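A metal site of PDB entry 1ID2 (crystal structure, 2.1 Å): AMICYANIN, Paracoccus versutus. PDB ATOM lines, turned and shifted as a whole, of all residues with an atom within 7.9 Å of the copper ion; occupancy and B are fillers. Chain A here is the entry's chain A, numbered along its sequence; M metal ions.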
ATOM      1  N   ILE A  26      14.565  -0.716 -24.790  1.00  0.00           N
ATOM      2  CA  ILE A  26      13.631   0.390 -24.737  1.00  0.00           C
ATOM      3  C   ILE A  26      12.847   0.352 -23.424  1.00  0.00           C
ATOM      4  O   ILE A  26      12.046  -0.563 -23.204  1.00  0.00           O
ATOM      5  CB  ILE A  26      12.646   0.356 -25.940  1.00  0.00           C
ATOM      6  CG1 ILE A  26      13.411   0.143 -27.264  1.00  0.00           C
ATOM      7  CG2 ILE A  26      11.881   1.674 -25.991  1.00  0.00           C
ATOM      8  CD1 ILE A  26      12.539  -0.260 -28.451  1.00  0.00           C
ATOM      9  N   MET A  29      10.019   5.255 -22.112  1.00  0.00           N
ATOM     10  CA  MET A  29       9.959   6.168 -23.238  1.00  0.00           C
ATOM     11  C   MET A  29      11.341   6.623 -23.707  1.00  0.00           C
ATOM     12  O   MET A  29      11.460   7.689 -24.294  1.00  0.00           O
ATOM     13  CB  MET A  29       9.100   7.385 -22.894  1.00  0.00           C
ATOM     14  CG  MET A  29       7.727   7.042 -22.341  1.00  0.00           C
ATOM     15  SD  MET A  29       6.654   6.187 -23.467  1.00  0.00           S
ATOM     16  CE  MET A  29       5.930   7.533 -24.409  1.00  0.00           C
ATOM     17  N   LYS A  30      12.346   5.765 -23.524  1.00  0.00           N
ATOM     18  CA  LYS A  30      13.721   6.068 -23.953  1.00  0.00           C
ATOM     19  C   LYS A  30      14.281   4.854 -24.679  1.00  0.00           C
ATOM     20  O   LYS A  30      14.044   3.722 -24.274  1.00  0.00           O
ATOM     21  CB  LYS A  30      14.628   6.303 -22.739  1.00  0.00           C
ATOM     22  CG  LYS A  30      14.483   7.625 -22.025  1.00  0.00           C
ATOM     23  CD  LYS A  30      15.022   7.530 -20.594  1.00  0.00           C
ATOM     24  CE  LYS A  30      16.538   7.346 -20.554  1.00  0.00           C
ATOM     25  NZ  LYS A  30      17.034   7.107 -19.163  1.00  0.00           N
ATOM     26  N   TYR A  31      15.142   5.099 -25.645  1.00  0.00           N
ATOM     27  CA  TYR A  31      16.063   4.082 -26.130  1.00  0.00           C
ATOM     28  C   TYR A  31      17.194   4.133 -25.153  1.00  0.00           C
ATOM     29  O   TYR A  31      17.797   5.179 -24.977  1.00  0.00           O
ATOM     30  CB  TYR A  31      16.605   4.452 -27.510  1.00  0.00           C
ATOM     31  CG  TYR A  31      15.556   4.449 -28.569  1.00  0.00           C
ATOM     32  CD1 TYR A  31      14.942   3.250 -28.960  1.00  0.00           C
ATOM     33  CD2 TYR A  31      15.144   5.636 -29.137  1.00  0.00           C
ATOM     34  CE1 TYR A  31      13.936   3.248 -29.918  1.00  0.00           C
ATOM     35  CE2 TYR A  31      14.139   5.642 -30.089  1.00  0.00           C
ATOM     36  CZ  TYR A  31      13.548   4.460 -30.486  1.00  0.00           C
ATOM     37  OH  TYR A  31      12.613   4.517 -31.509  1.00  0.00           O
ATOM     38  N   ASN A  48      11.764  -4.026 -26.812  1.00  0.00           N
ATOM     39  CA  ASN A  48      10.870  -3.203 -26.042  1.00  0.00           C
ATOM     40  C   ASN A  48      10.563  -3.868 -24.698  1.00  0.00           C
ATOM     41  O   ASN A  48      10.053  -4.998 -24.656  1.00  0.00           O
ATOM     42  CB  ASN A  48       9.554  -2.970 -26.814  1.00  0.00           C
ATOM     43  CG  ASN A  48       8.629  -1.992 -26.105  1.00  0.00           C
ATOM     44  OD1 ASN A  48       9.048  -1.327 -25.181  1.00  0.00           O
ATOM     45  ND2 ASN A  48       7.376  -1.907 -26.537  1.00  0.00           N
ATOM     46  N   GLU A  50       8.542  -2.483 -22.338  1.00  0.00           N
ATOM     47  CA  GLU A  50       7.323  -1.984 -21.702  1.00  0.00           C
ATOM     48  C   GLU A  50       6.085  -2.207 -22.542  1.00  0.00           C
ATOM     49  O   GLU A  50       6.181  -2.493 -23.734  1.00  0.00           O
ATOM     50  CB  GLU A  50       7.478  -0.501 -21.345  1.00  0.00           C
ATOM     51  CG  GLU A  50       8.019   0.417 -22.442  1.00  0.00           C
ATOM     52  CD  GLU A  50       8.287   1.843 -21.956  1.00  0.00           C
ATOM     53  OE1 GLU A  50       8.512   2.031 -20.748  1.00  0.00           O
ATOM     54  OE2 GLU A  50       8.318   2.764 -22.786  1.00  0.00           O
ATOM     55  N   MET A  52       3.851   0.118 -23.567  1.00  0.00           N
ATOM     56  CA  MET A  52       3.762   1.123 -24.633  1.00  0.00           C
ATOM     57  C   MET A  52       4.427   0.609 -25.899  1.00  0.00           C
ATOM     58  O   MET A  52       5.607   0.304 -25.899  1.00  0.00           O
ATOM     59  CB  MET A  52       4.475   2.405 -24.219  1.00  0.00           C
ATOM     60  CG  MET A  52       4.349   3.543 -25.213  1.00  0.00           C
ATOM     61  SD  MET A  52       2.735   4.307 -25.150  1.00  0.00           S
ATOM     62  CE  MET A  52       2.991   5.556 -23.873  1.00  0.00           C
ATOM     63  N   PRO A  53       3.721   0.638 -27.018  1.00  0.00           N
ATOM     64  CA  PRO A  53       4.400   0.113 -28.199  1.00  0.00           C
ATOM     65  C   PRO A  53       5.379   1.145 -28.753  1.00  0.00           C
ATOM     66  O   PRO A  53       5.115   2.349 -28.712  1.00  0.00           O
ATOM     67  CB  PRO A  53       3.252  -0.199 -29.155  1.00  0.00           C
ATOM     68  CG  PRO A  53       2.037  -0.332 -28.243  1.00  0.00           C
ATOM     69  CD  PRO A  53       2.266   0.737 -27.229  1.00  0.00           C
ATOM     70  N   HIS A  54       6.480   0.656 -29.300  1.00  0.00           N
ATOM     71  CA  HIS A  54       7.551   1.483 -29.825  1.00  0.00           C
ATOM     72  C   HIS A  54       8.052   0.860 -31.113  1.00  0.00           C
ATOM     73  O   HIS A  54       7.949  -0.349 -31.283  1.00  0.00           O
ATOM     74  CB  HIS A  54       8.672   1.591 -28.810  1.00  0.00           C
ATOM     75  CG  HIS A  54       8.283   2.282 -27.531  1.00  0.00           C
ATOM     76  ND1 HIS A  54       7.913   3.602 -27.498  1.00  0.00           N
ATOM     77  CD2 HIS A  54       8.352   1.817 -26.256  1.00  0.00           C
ATOM     78  CE1 HIS A  54       7.764   3.915 -26.225  1.00  0.00           C
ATOM     79  NE2 HIS A  54       8.013   2.880 -25.440  1.00  0.00           N
ATOM     80  N   ASN A  55       8.434   1.685 -32.081  1.00  0.00           N
ATOM     81  CA  ASN A  55       9.078   1.167 -33.291  1.00  0.00           C
ATOM     82  C   ASN A  55      10.386   1.887 -33.564  1.00  0.00           C
ATOM     83  O   ASN A  55      10.909   2.589 -32.673  1.00  0.00           O
ATOM     84  CB  ASN A  55       8.143   1.268 -34.510  1.00  0.00           C
ATOM     85  CG  ASN A  55       8.055   2.665 -35.077  1.00  0.00           C
ATOM     86  OD1 ASN A  55       8.241   3.625 -34.357  1.00  0.00           O
ATOM     87  ND2 ASN A  55       7.655   2.792 -36.346  1.00  0.00           N
ATOM     88  N   VAL A  56      11.024   1.528 -34.686  1.00  0.00           N
ATOM     89  CA  VAL A  56      12.242   2.210 -35.163  1.00  0.00           C
ATOM     90  C   VAL A  56      11.936   2.753 -36.548  1.00  0.00           C
ATOM     91  O   VAL A  56      11.376   2.023 -37.367  1.00  0.00           O
ATOM     92  CB  VAL A  56      13.447   1.212 -35.228  1.00  0.00           C
ATOM     93  CG1 VAL A  56      14.637   1.843 -35.926  1.00  0.00           C
ATOM     94  CG2 VAL A  56      13.855   0.835 -33.835  1.00  0.00           C
ATOM     95  N   MET A  72       5.519  -1.835 -35.094  1.00  0.00           N
ATOM     96  CA  MET A  72       5.454  -1.636 -33.628  1.00  0.00           C
ATOM     97  C   MET A  72       5.749  -2.913 -32.816  1.00  0.00           C
ATOM     98  O   MET A  72       5.266  -3.983 -33.165  1.00  0.00           O
ATOM     99  CB  MET A  72       4.077  -1.104 -33.226  1.00  0.00           C
ATOM    100  CG  MET A  72       3.633   0.156 -33.964  1.00  0.00           C
ATOM    101  SD  MET A  72       4.693   1.577 -33.672  1.00  0.00           S
ATOM    102  CE  MET A  72       4.528   1.644 -31.974  1.00  0.00           C
ATOM    103  N   MET A  73       6.619  -2.791 -31.820  1.00  0.00           N
ATOM    104  CA  MET A  73       6.892  -3.861 -30.851  1.00  0.00           C
ATOM    105  C   MET A  73       6.026  -3.579 -29.657  1.00  0.00           C
ATOM    106  O   MET A  73       5.799  -2.411 -29.278  1.00  0.00           O
ATOM    107  CB  MET A  73       8.350  -3.862 -30.366  1.00  0.00           C
ATOM    108  CG  MET A  73       9.406  -4.128 -31.409  1.00  0.00           C
ATOM    109  SD  MET A  73      11.080  -3.578 -30.934  1.00  0.00           S
ATOM    110  CE  MET A  73      11.203  -2.006 -31.811  1.00  0.00           C
ATOM    111  N   PHE A  92      13.907   7.412 -34.876  1.00  0.00           N
ATOM    112  CA  PHE A  92      13.006   7.937 -33.882  1.00  0.00           C
ATOM    113  C   PHE A  92      11.831   6.975 -33.837  1.00  0.00           C
ATOM    114  O   PHE A  92      11.744   6.038 -34.640  1.00  0.00           O
ATOM    115  CB  PHE A  92      12.552   9.366 -34.274  1.00  0.00           C
ATOM    116  CG  PHE A  92      11.870   9.431 -35.613  1.00  0.00           C
ATOM    117  CD1 PHE A  92      12.610   9.396 -36.790  1.00  0.00           C
ATOM    118  CD2 PHE A  92      10.478   9.394 -35.704  1.00  0.00           C
ATOM    119  CE1 PHE A  92      11.982   9.310 -38.022  1.00  0.00           C
ATOM    120  CE2 PHE A  92       9.850   9.300 -36.942  1.00  0.00           C
ATOM    121  CZ  PHE A  92      10.617   9.255 -38.105  1.00  0.00           C
ATOM    122  N   CYS A  93      10.952   7.160 -32.868  1.00  0.00           N
ATOM    123  CA  CYS A  93       9.799   6.307 -32.699  1.00  0.00           C
ATOM    124  C   CYS A  93       8.634   7.070 -33.248  1.00  0.00           C
ATOM    125  O   CYS A  93       8.463   8.239 -32.955  1.00  0.00           O
ATOM    126  CB  CYS A  93       9.594   5.995 -31.211  1.00  0.00           C
ATOM    127  SG  CYS A  93       8.122   5.049 -30.932  1.00  0.00           S
ATOM    128  N   THR A  94       7.940   6.464 -34.205  1.00  0.00           N
ATOM    129  CA  THR A  94       6.981   7.161 -35.037  1.00  0.00           C
ATOM    130  C   THR A  94       5.909   7.914 -34.240  1.00  0.00           C
ATOM    131  O   THR A  94       5.654   9.078 -34.503  1.00  0.00           O
ATOM    132  CB  THR A  94       6.304   6.165 -36.018  1.00  0.00           C
ATOM    133  OG1 THR A  94       7.286   5.676 -36.925  1.00  0.00           O
ATOM    134  CG2 THR A  94       5.181   6.843 -36.806  1.00  0.00           C
ATOM    135  N   PRO A  95       5.270   7.254 -33.261  1.00  0.00           N
ATOM    136  CA  PRO A  95       4.263   7.993 -32.495  1.00  0.00           C
ATOM    137  C   PRO A  95       4.843   8.861 -31.355  1.00  0.00           C
ATOM    138  O   PRO A  95       4.146   9.716 -30.800  1.00  0.00           O
ATOM    139  CB  PRO A  95       3.362   6.877 -31.980  1.00  0.00           C
ATOM    140  CG  PRO A  95       4.309   5.749 -31.781  1.00  0.00           C
ATOM    141  CD  PRO A  95       5.227   5.815 -32.961  1.00  0.00           C
ATOM    142  N   HIS A  96       6.136   8.703 -31.079  1.00  0.00           N
ATOM    143  CA  HIS A  96       6.825   9.387 -29.992  1.00  0.00           C
ATOM    144  C   HIS A  96       8.129   9.962 -30.509  1.00  0.00           C
ATOM    145  O   HIS A  96       9.222   9.469 -30.164  1.00  0.00           O
ATOM    146  CB  HIS A  96       7.129   8.403 -28.851  1.00  0.00           C
ATOM    147  CG  HIS A  96       5.955   7.544 -28.453  1.00  0.00           C
ATOM    148  ND1 HIS A  96       6.077   6.184 -28.329  1.00  0.00           N
ATOM    149  CD2 HIS A  96       4.664   7.910 -28.249  1.00  0.00           C
ATOM    150  CE1 HIS A  96       4.865   5.738 -28.059  1.00  0.00           C
ATOM    151  NE2 HIS A  96       3.970   6.745 -28.005  1.00  0.00           N
ATOM    152  N   PRO A  97       8.058  10.995 -31.374  1.00  0.00           N
ATOM    153  CA  PRO A  97       9.227  11.485 -32.116  1.00  0.00           C
ATOM    154  C   PRO A  97      10.279  12.164 -31.224  1.00  0.00           C
ATOM    155  O   PRO A  97      11.350  12.516 -31.689  1.00  0.00           O
ATOM    156  CB  PRO A  97       8.622  12.479 -33.117  1.00  0.00           C
ATOM    157  CG  PRO A  97       7.143  12.395 -32.923  1.00  0.00           C
ATOM    158  CD  PRO A  97       6.907  11.879 -31.579  1.00  0.00           C
ATOM    159  N   PHE A  98       9.955  12.373 -29.961  1.00  0.00           N
ATOM    160  CA  PHE A  98      10.926  12.883 -29.024  1.00  0.00           C
ATOM    161  C   PHE A  98      11.883  11.780 -28.638  1.00  0.00           C
ATOM    162  O   PHE A  98      12.885  12.049 -27.981  1.00  0.00           O
ATOM    163  CB  PHE A  98      10.224  13.400 -27.779  1.00  0.00           C
ATOM    164  CG  PHE A  98       9.253  12.425 -27.169  1.00  0.00           C
ATOM    165  CD1 PHE A  98       9.670  11.504 -26.217  1.00  0.00           C
ATOM    166  CD2 PHE A  98       7.918  12.407 -27.559  1.00  0.00           C
ATOM    167  CE1 PHE A  98       8.801  10.599 -25.668  1.00  0.00           C
ATOM    168  CE2 PHE A  98       7.014  11.510 -26.988  1.00  0.00           C
ATOM    169  CZ  PHE A  98       7.466  10.597 -26.047  1.00  0.00           C
ATOM    170  N   MET A  99      11.479  10.528 -28.871  1.00  0.00           N
ATOM    171  CA  MET A  99      12.386   9.364 -28.758  1.00  0.00           C
ATOM    172  C   MET A  99      13.262   9.246 -30.008  1.00  0.00           C
ATOM    173  O   MET A  99      12.760   9.052 -31.107  1.00  0.00           O
ATOM    174  CB  MET A  99      11.598   8.055 -28.606  1.00  0.00           C
ATOM    175  CG  MET A  99      10.865   7.864 -27.287  1.00  0.00           C
ATOM    176  SD  MET A  99       9.920   6.318 -27.286  1.00  0.00           S
ATOM    177  CE  MET A  99      11.292   5.129 -27.103  1.00  0.00           C
HETATM  178 CU    CU M   1       7.890   5.060 -28.901  1.00  0.00          CU
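A ring nitrogen (NE2) of His 54 sits at hydrogen-bond distance from the side-chain carboxylate (OE2) of Glu 50, 2.7 Å away.
N of Met 73 is in hydrogen-bond range of O of His 54, 2.8 Å away.
The side-chain hydroxyl of Tyr 31 sits close to the backbone NH of Cys 93.
N of Asn 55 sits close to SG of Cys 93 (3.6 Å).
The side-chain sulfur (SD) of Met 99 lies close to a ring nitrogen (ND1) of His 54, 3.4 Å away.
N of Cys 93 lies within hydrogen-bond range of O of Met 99, at 3.2 Å.
Merely in contact with the copper ion: Pro 53 (3.9 Å).
Of the 21 residues printed, 5 come within 4 Å of the copper ion.
The copper ion is bound by ND1 of His 54, SG of Cys 93 and ND1 of His 96.
Slightly farther from the copper ion lies the side-chain sulfur (SD) of Met 99 (2.9 Å).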
